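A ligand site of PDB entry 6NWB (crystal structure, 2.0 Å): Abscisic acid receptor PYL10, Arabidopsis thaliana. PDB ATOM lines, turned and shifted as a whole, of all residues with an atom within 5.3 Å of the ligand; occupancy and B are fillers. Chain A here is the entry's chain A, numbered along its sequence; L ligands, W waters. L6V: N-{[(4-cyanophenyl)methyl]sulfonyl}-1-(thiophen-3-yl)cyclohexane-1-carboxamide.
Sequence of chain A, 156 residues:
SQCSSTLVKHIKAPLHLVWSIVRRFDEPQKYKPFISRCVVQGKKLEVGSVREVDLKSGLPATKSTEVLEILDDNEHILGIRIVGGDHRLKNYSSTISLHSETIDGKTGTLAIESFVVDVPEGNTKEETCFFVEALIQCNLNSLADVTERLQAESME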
ATOM      1  N   LYS A  32       8.635   1.770   9.923  1.00  0.00           N
ATOM      2  CA  LYS A  32       8.837   2.568  11.130  1.00  0.00           C
ATOM      3  C   LYS A  32       9.374   1.701  12.262  1.00  0.00           C
ATOM      4  O   LYS A  32       8.666   0.816  12.764  1.00  0.00           O
ATOM      5  CB  LYS A  32       7.531   3.266  11.544  1.00  0.00           C
ATOM      6  CG  LYS A  32       7.171   4.441  10.648  1.00  0.00           C
ATOM      7  CD  LYS A  32       5.881   5.067  11.133  1.00  0.00           C
ATOM      8  CE  LYS A  32       5.820   6.552  10.901  1.00  0.00           C
ATOM      9  NZ  LYS A  32       4.685   7.098  11.714  1.00  0.00           N
ATOM     10  N   PHE A  34       9.959   2.161  15.392  1.00  0.00           N
ATOM     11  CA  PHE A  34       9.497   2.338  16.770  1.00  0.00           C
ATOM     12  C   PHE A  34       8.091   1.789  16.985  1.00  0.00           C
ATOM     13  O   PHE A  34       7.541   1.946  18.079  1.00  0.00           O
ATOM     14  CB  PHE A  34       9.598   3.814  17.147  1.00  0.00           C
ATOM     15  CG  PHE A  34      11.009   4.348  17.092  1.00  0.00           C
ATOM     16  CD1 PHE A  34      12.052   3.592  17.568  1.00  0.00           C
ATOM     17  CD2 PHE A  34      11.286   5.578  16.538  1.00  0.00           C
ATOM     18  CE1 PHE A  34      13.350   4.061  17.508  1.00  0.00           C
ATOM     19  CE2 PHE A  34      12.591   6.052  16.479  1.00  0.00           C
ATOM     20  CZ  PHE A  34      13.618   5.284  16.973  1.00  0.00           C
ATOM     21  N   ILE A  35       7.511   1.145  15.970  1.00  0.00           N
ATOM     22  CA  ILE A  35       6.190   0.530  16.049  1.00  0.00           C
ATOM     23  C   ILE A  35       6.360  -0.974  16.206  1.00  0.00           C
ATOM     24  O   ILE A  35       7.022  -1.620  15.391  1.00  0.00           O
ATOM     25  CB  ILE A  35       5.366   0.836  14.786  1.00  0.00           C
ATOM     26  CG1 ILE A  35       5.286   2.330  14.534  1.00  0.00           C
ATOM     27  CG2 ILE A  35       3.977   0.206  14.903  1.00  0.00           C
ATOM     28  CD1 ILE A  35       4.661   3.072  15.651  1.00  0.00           C
ATOM     29  N   ARG A  51      -6.149   3.825  13.130  1.00  0.00           N
ATOM     30  CA  ARG A  51      -5.161   2.840  13.524  1.00  0.00           C
ATOM     31  C   ARG A  51      -4.743   3.089  14.964  1.00  0.00           C
ATOM     32  O   ARG A  51      -4.622   4.236  15.394  1.00  0.00           O
ATOM     33  CB  ARG A  51      -3.917   2.866  12.603  1.00  0.00           C
ATOM     34  CG  ARG A  51      -2.938   4.015  12.794  1.00  0.00           C
ATOM     35  CD  ARG A  51      -1.906   4.027  11.672  1.00  0.00           C
ATOM     36  NE  ARG A  51      -0.862   5.034  11.828  1.00  0.00           N
ATOM     37  CZ  ARG A  51       0.046   5.315  10.899  1.00  0.00           C
ATOM     38  NH1 ARG A  51       0.964   6.236  11.138  1.00  0.00           N
ATOM     39  NH2 ARG A  51       0.030   4.684   9.730  1.00  0.00           N
ATOM     40  N   LEU A  55       3.824   1.114  20.687  1.00  0.00           N
ATOM     41  CA  LEU A  55       5.211   1.481  20.472  1.00  0.00           C
ATOM     42  C   LEU A  55       6.147   0.438  21.084  1.00  0.00           C
ATOM     43  O   LEU A  55       5.774  -0.326  21.971  1.00  0.00           O
ATOM     44  CB  LEU A  55       5.527   2.856  21.040  1.00  0.00           C
ATOM     45  CG  LEU A  55       4.598   3.977  20.608  1.00  0.00           C
ATOM     46  CD1 LEU A  55       5.080   5.270  21.225  1.00  0.00           C
ATOM     47  CD2 LEU A  55       4.532   4.061  19.083  1.00  0.00           C
ATOM     48  N   LEU A  59      10.329   2.882  25.358  1.00  0.00           N
ATOM     49  CA  LEU A  59      10.132   4.217  24.820  1.00  0.00           C
ATOM     50  C   LEU A  59       9.406   5.090  25.821  1.00  0.00           C
ATOM     51  O   LEU A  59       8.793   4.586  26.775  1.00  0.00           O
ATOM     52  CB  LEU A  59       9.357   4.148  23.501  1.00  0.00           C
ATOM     53  CG  LEU A  59      10.289   4.270  22.304  1.00  0.00           C
ATOM     54  CD1 LEU A  59      11.393   3.223  22.394  1.00  0.00           C
ATOM     55  CD2 LEU A  59       9.528   4.136  20.997  1.00  0.00           C
ATOM     56  N   PRO A  60       9.459   6.414  25.666  1.00  0.00           N
ATOM     57  CA  PRO A  60       8.751   7.299  26.608  1.00  0.00           C
ATOM     58  C   PRO A  60       7.241   7.329  26.414  1.00  0.00           C
ATOM     59  O   PRO A  60       6.563   8.062  27.128  1.00  0.00           O
ATOM     60  CB  PRO A  60       9.371   8.663  26.320  1.00  0.00           C
ATOM     61  CG  PRO A  60       9.739   8.574  24.866  1.00  0.00           C
ATOM     62  CD  PRO A  60      10.257   7.183  24.689  1.00  0.00           C
ATOM     63  N   ALA A  61       6.706   6.595  25.441  1.00  0.00           N
ATOM     64  CA  ALA A  61       5.270   6.405  25.293  1.00  0.00           C
ATOM     65  C   ALA A  61       5.031   4.958  24.889  1.00  0.00           C
ATOM     66  O   ALA A  61       5.971   4.212  24.598  1.00  0.00           O
ATOM     67  CB  ALA A  61       4.676   7.383  24.257  1.00  0.00           C
ATOM     68  N   SER A  64      -0.424   5.078  20.409  1.00  0.00           N
ATOM     69  CA  SER A  64      -0.901   6.230  19.678  1.00  0.00           C
ATOM     70  C   SER A  64      -2.139   5.798  18.900  1.00  0.00           C
ATOM     71  O   SER A  64      -2.257   4.629  18.510  1.00  0.00           O
ATOM     72  CB  SER A  64       0.180   6.806  18.756  1.00  0.00           C
ATOM     73  OG  SER A  64      -0.182   8.088  18.271  1.00  0.00           O
ATOM     74  N   GLU A  66      -4.387   7.161  15.539  1.00  0.00           N
ATOM     75  CA  GLU A  66      -4.149   8.025  14.405  1.00  0.00           C
ATOM     76  C   GLU A  66      -5.208   7.801  13.323  1.00  0.00           C
ATOM     77  O   GLU A  66      -5.679   6.677  13.117  1.00  0.00           O
ATOM     78  CB  GLU A  66      -2.715   7.796  13.865  1.00  0.00           C
ATOM     79  CG  GLU A  66      -1.657   8.247  14.875  1.00  0.00           C
ATOM     80  CD  GLU A  66      -0.273   7.598  14.725  1.00  0.00           C
ATOM     81  OE1 GLU A  66       0.589   7.870  15.596  1.00  0.00           O
ATOM     82  OE2 GLU A  66      -0.043   6.826  13.759  1.00  0.00           O
ATOM     83  N   ILE A  80      -1.987  12.338   7.847  1.00  0.00           N
ATOM     84  CA  ILE A  80      -2.379  11.612   9.064  1.00  0.00           C
ATOM     85  C   ILE A  80      -2.450  12.572  10.236  1.00  0.00           C
ATOM     86  O   ILE A  80      -1.633  13.496  10.361  1.00  0.00           O
ATOM     87  CB  ILE A  80      -1.396  10.464   9.358  1.00  0.00           C
ATOM     88  CG1 ILE A  80      -1.375   9.451   8.224  1.00  0.00           C
ATOM     89  CG2 ILE A  80      -1.749   9.733  10.637  1.00  0.00           C
ATOM     90  CD1 ILE A  80      -0.243   8.430   8.344  1.00  0.00           C
ATOM     91  N   ILE A  82      -2.848  12.638  14.582  1.00  0.00           N
ATOM     92  CA  ILE A  82      -2.825  11.890  15.839  1.00  0.00           C
ATOM     93  C   ILE A  82      -3.960  12.400  16.702  1.00  0.00           C
ATOM     94  O   ILE A  82      -4.046  13.604  16.971  1.00  0.00           O
ATOM     95  CB  ILE A  82      -1.483  12.055  16.564  1.00  0.00           C
ATOM     96  CG1 ILE A  82      -0.344  11.473  15.741  1.00  0.00           C
ATOM     97  CG2 ILE A  82      -1.552  11.366  17.936  1.00  0.00           C
ATOM     98  CD1 ILE A  82       0.978  11.584  16.455  1.00  0.00           C
ATOM     99  N   HIS A  87       1.671   9.675  24.509  1.00  0.00           N
ATOM    100  CA  HIS A  87       2.738  10.629  24.245  1.00  0.00           C
ATOM    101  C   HIS A  87       2.227  12.041  24.483  1.00  0.00           C
ATOM    102  O   HIS A  87       1.029  12.266  24.714  1.00  0.00           O
ATOM    103  CB  HIS A  87       3.233  10.477  22.828  1.00  0.00           C
ATOM    104  CG  HIS A  87       2.144  10.541  21.814  1.00  0.00           C
ATOM    105  ND1 HIS A  87       1.445  11.702  21.563  1.00  0.00           N
ATOM    106  CD2 HIS A  87       1.576   9.583  21.041  1.00  0.00           C
ATOM    107  CE1 HIS A  87       0.518  11.464  20.649  1.00  0.00           C
ATOM    108  NE2 HIS A  87       0.578  10.185  20.318  1.00  0.00           N
ATOM    109  N   LEU A  89       2.140  14.622  22.472  1.00  0.00           N
ATOM    110  CA  LEU A  89       1.814  15.360  21.260  1.00  0.00           C
ATOM    111  C   LEU A  89       0.297  15.490  21.116  1.00  0.00           C
ATOM    112  O   LEU A  89      -0.431  14.500  21.066  1.00  0.00           O
ATOM    113  CB  LEU A  89       2.390  14.652  20.041  1.00  0.00           C
ATOM    114  CG  LEU A  89       3.898  14.380  20.065  1.00  0.00           C
ATOM    115  CD1 LEU A  89       4.293  13.791  18.746  1.00  0.00           C
ATOM    116  CD2 LEU A  89       4.686  15.649  20.347  1.00  0.00           C
ATOM    117  N   TYR A  92      -1.326  16.895  16.574  1.00  0.00           N
ATOM    118  CA  TYR A  92      -0.262  16.619  15.616  1.00  0.00           C
ATOM    119  C   TYR A  92      -0.885  16.222  14.276  1.00  0.00           C
ATOM    120  O   TYR A  92      -1.704  15.312  14.222  1.00  0.00           O
ATOM    121  CB  TYR A  92       0.643  15.508  16.137  1.00  0.00           C
ATOM    122  CG  TYR A  92       1.829  15.191  15.235  1.00  0.00           C
ATOM    123  CD1 TYR A  92       1.683  14.417  14.091  1.00  0.00           C
ATOM    124  CD2 TYR A  92       3.107  15.648  15.544  1.00  0.00           C
ATOM    125  CE1 TYR A  92       2.759  14.119  13.273  1.00  0.00           C
ATOM    126  CE2 TYR A  92       4.192  15.370  14.737  1.00  0.00           C
ATOM    127  CZ  TYR A  92       4.018  14.599  13.602  1.00  0.00           C
ATOM    128  OH  TYR A  92       5.109  14.313  12.806  1.00  0.00           O
ATOM    129  N   SER A  94       0.446  15.227  10.272  1.00  0.00           N
ATOM    130  CA  SER A  94       1.587  14.801   9.468  1.00  0.00           C
ATOM    131  C   SER A  94       1.205  14.748   7.998  1.00  0.00           C
ATOM    132  O   SER A  94       0.095  14.324   7.657  1.00  0.00           O
ATOM    133  CB  SER A  94       2.067  13.421   9.930  1.00  0.00           C
ATOM    134  OG  SER A  94       2.897  12.801   8.952  1.00  0.00           O
ATOM    135  N   GLU A 113       8.589  15.046   4.510  1.00  0.00           N
ATOM    136  CA  GLU A 113       7.628  14.870   5.586  1.00  0.00           C
ATOM    137  C   GLU A 113       7.556  16.137   6.426  1.00  0.00           C
ATOM    138  O   GLU A 113       8.577  16.613   6.944  1.00  0.00           O
ATOM    139  CB  GLU A 113       7.963  13.648   6.450  1.00  0.00           C
ATOM    140  CG  GLU A 113       6.948  13.456   7.583  1.00  0.00           C
ATOM    141  CD  GLU A 113       6.971  12.075   8.233  1.00  0.00           C
ATOM    142  OE1 GLU A 113       7.677  11.169   7.732  1.00  0.00           O
ATOM    143  OE2 GLU A 113       6.268  11.886   9.251  1.00  0.00           O
ATOM    144  N   PHE A 131      12.839  17.723  18.778  1.00  0.00           N
ATOM    145  CA  PHE A 131      12.529  16.341  19.111  1.00  0.00           C
ATOM    146  C   PHE A 131      11.807  15.641  17.958  1.00  0.00           C
ATOM    147  O   PHE A 131      12.208  14.568  17.513  1.00  0.00           O
ATOM    148  CB  PHE A 131      11.688  16.323  20.392  1.00  0.00           C
ATOM    149  CG  PHE A 131      11.315  14.962  20.882  1.00  0.00           C
ATOM    150  CD1 PHE A 131      12.240  14.197  21.582  1.00  0.00           C
ATOM    151  CD2 PHE A 131      10.034  14.470  20.692  1.00  0.00           C
ATOM    152  CE1 PHE A 131      11.893  12.947  22.063  1.00  0.00           C
ATOM    153  CE2 PHE A 131       9.688  13.220  21.163  1.00  0.00           C
ATOM    154  CZ  PHE A 131      10.621  12.461  21.854  1.00  0.00           C
ATOM    155  N   VAL A 132      10.753  16.284  17.453  1.00  0.00           N
ATOM    156  CA  VAL A 132       9.974  15.683  16.378  1.00  0.00           C
ATOM    157  C   VAL A 132      10.813  15.559  15.117  1.00  0.00           C
ATOM    158  O   VAL A 132      10.723  14.565  14.398  1.00  0.00           O
ATOM    159  CB  VAL A 132       8.698  16.492  16.111  1.00  0.00           C
ATOM    160  CG1 VAL A 132       7.932  15.910  14.956  1.00  0.00           C
ATOM    161  CG2 VAL A 132       7.823  16.534  17.360  1.00  0.00           C
ATOM    162  N   LEU A 135      13.023  12.498  15.202  1.00  0.00           N
ATOM    163  CA  LEU A 135      12.242  11.278  15.021  1.00  0.00           C
ATOM    164  C   LEU A 135      11.829  11.072  13.570  1.00  0.00           C
ATOM    165  O   LEU A 135      11.961   9.970  13.022  1.00  0.00           O
ATOM    166  CB  LEU A 135      11.035  11.334  15.943  1.00  0.00           C
ATOM    167  CG  LEU A 135      10.136  10.120  16.006  1.00  0.00           C
ATOM    168  CD1 LEU A 135      10.972   8.873  15.894  1.00  0.00           C
ATOM    169  CD2 LEU A 135       9.396  10.134  17.342  1.00  0.00           C
ATOM    170  N   ILE A 136      11.337  12.125  12.920  1.00  0.00           N
ATOM    171  CA  ILE A 136      10.965  11.993  11.521  1.00  0.00           C
ATOM    172  C   ILE A 136      12.195  11.650  10.681  1.00  0.00           C
ATOM    173  O   ILE A 136      12.166  10.764   9.814  1.00  0.00           O
ATOM    174  CB  ILE A 136      10.269  13.274  11.039  1.00  0.00           C
ATOM    175  CG1 ILE A 136       8.931  13.408  11.754  1.00  0.00           C
ATOM    176  CG2 ILE A 136      10.048  13.247   9.527  1.00  0.00           C
ATOM    177  CD1 ILE A 136       8.211  14.663  11.412  1.00  0.00           C
ATOM    178  N   ASN A 139      12.842   8.056  11.003  1.00  0.00           N
ATOM    179  CA  ASN A 139      11.876   7.304  10.220  1.00  0.00           C
ATOM    180  C   ASN A 139      12.159   7.401   8.721  1.00  0.00           C
ATOM    181  O   ASN A 139      12.025   6.398   8.009  1.00  0.00           O
ATOM    182  CB  ASN A 139      10.460   7.794  10.539  1.00  0.00           C
ATOM    183  CG  ASN A 139      10.029   7.392  11.932  1.00  0.00           C
ATOM    184  OD1 ASN A 139      10.618   6.505  12.536  1.00  0.00           O
ATOM    185  ND2 ASN A 139       8.974   8.028  12.448  1.00  0.00           N
HETATM  186  CAA L6V L   1       7.607   6.981  18.645  1.00  0.00           C
HETATM  187  CAB L6V L   1       6.382   6.938  17.985  1.00  0.00           C
HETATM  188  CAC L6V L   1       5.320   7.732  18.399  1.00  0.00           C
HETATM  189  CAD L6V L   1       5.505   8.588  19.495  1.00  0.00           C
HETATM  190  CAE L6V L   1       6.730   8.630  20.155  1.00  0.00           C
HETATM  191  CAF L6V L   1       7.785   7.830  19.730  1.00  0.00           C
HETATM  192  CAG L6V L   1       6.917   9.514  21.280  1.00  0.00           C
HETATM  193  CAI L6V L   1       6.212   5.988  16.811  1.00  0.00           C
HETATM  194  CAL L6V L   1       5.823   9.006  14.192  1.00  0.00           C
HETATM  195  CAO L6V L   1       5.017  10.300  14.245  1.00  0.00           C
HETATM  196  CAP L6V L   1       3.784  10.137  13.336  1.00  0.00           C
HETATM  197  CAR L6V L   1       2.675  10.124  11.259  1.00  0.00           C
HETATM  198  CAS L6V L   1       3.839  10.322  11.885  1.00  0.00           C
HETATM  199  CAT L6V L   1       2.585   9.779  13.800  1.00  0.00           C
HETATM  200  CAU L6V L   1       6.679  12.046  15.998  1.00  0.00           C
HETATM  201  CAV L6V L   1       7.135  11.607  14.621  1.00  0.00           C
HETATM  202  CAW L6V L   1       5.928  11.413  13.713  1.00  0.00           C
HETATM  203  CAX L6V L   1       4.623  10.676  15.676  1.00  0.00           C
HETATM  204  CAY L6V L   1       5.803  10.965  16.613  1.00  0.00           C
HETATM  205  NAH L6V L   1       7.074  10.224  22.195  1.00  0.00           N
HETATM  206  NAK L6V L   1       5.708   8.201  15.252  1.00  0.00           N
HETATM  207  OAM L6V L   1       6.186   5.904  14.247  1.00  0.00           O
HETATM  208  OAN L6V L   1       7.984   7.138  15.358  1.00  0.00           O
HETATM  209  OAZ L6V L   1       6.487   8.752  13.184  1.00  0.00           O
HETATM  210  SAJ L6V L   1       6.598   6.786  15.283  1.00  0.00           S
HETATM  211  SAQ L6V L   1       1.568   9.693  12.440  1.00  0.00           S
HETATM  212  O   HOH W   1       9.256   4.658  14.012  1.00  0.00           O
HETATM  213  O   HOH W   2       7.572   9.803  10.728  1.00  0.00           O
HETATM  214  O   HOH W   3       3.061   6.808  16.193  1.00  0.00           O
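The side-chain amide nitrogen of Asn 139 lies within hydrogen-bond range of an oxygen (OAZ) of the ligand, at 2.7 Å.
OAZ of the ligand sits at hydrogen-bond distance from NZ of Lys 32 (2.9 Å).
SAQ of the ligand sits close to NH1 of Arg 51 (3.7 Å).
The backbone NH (N) of Ile 82 lies within hydrogen-bond range of the backbone carbonyl oxygen (O) of Tyr 92, at 2.9 Å.
OE2 of Glu 66 lies within salt-bridge range of NE of Arg 51, at 2.8 Å.
OE1 of Glu 66 is in hydrogen-bond range of OG of Ser 64, at 2.8 Å.
N of Ser 94 lies within hydrogen-bond range of O of Ile 80, 2.7 Å away.
A ring nitrogen (ND1) of His 87 lies within hydrogen-bond range of the backbone NH (N) of Leu 89 (3.1 Å).
NE2 of His 87 lies within hydrogen-bond range of OG of Ser 64, at 3.0 Å.
The side-chain carboxylate (OE2) of Glu 66 sits close to a sulfur (SAQ) of the ligand (3.5 Å).
Merely in contact with the ligand: Tyr 92 (3.1 Å), Leu 55 (3.4 Å), Leu 135 (3.5 Å), Ile 35 (3.5 Å), Ser 94 (3.5 Å), Ile 82 (3.6 Å), Ile 80 (3.8 Å), Ile 136 (3.8 Å), Phe 34 (3.8 Å), Leu 89 (3.8 Å), His 87 (3.9 Å) and Glu 113 (3.9 Å).
Hydrophobic or aromatic side chains that line the ligand: Phe 34, Ile 35, Leu 55, Ile 80, Ile 82, His 87, Leu 89, Tyr 92, Leu 135 and Ile 136.
The nearest printed residue that does not touch the ligand is Phe 131 (4.1 Å).
Water W2 lies within hydrogen-bond range of the side-chain amide nitrogen (ND2) of Asn 139 (2.8 Å), the side-chain carboxylate (OE2) of Glu 113 (2.9 Å) and an oxygen (OAZ) of the ligand (2.9 Å).
Water W1 lies within hydrogen-bond range of the side-chain amide oxygen (OD1) of Asn 139 (2.7 Å), the backbone NH (N) of Phe 34 (2.9 Å) and an oxygen (OAN) of the ligand (3.1 Å).
Water W3 bridges OE1 of Glu 66 (2.8 Å) and NAK of the ligand (3.1 Å).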
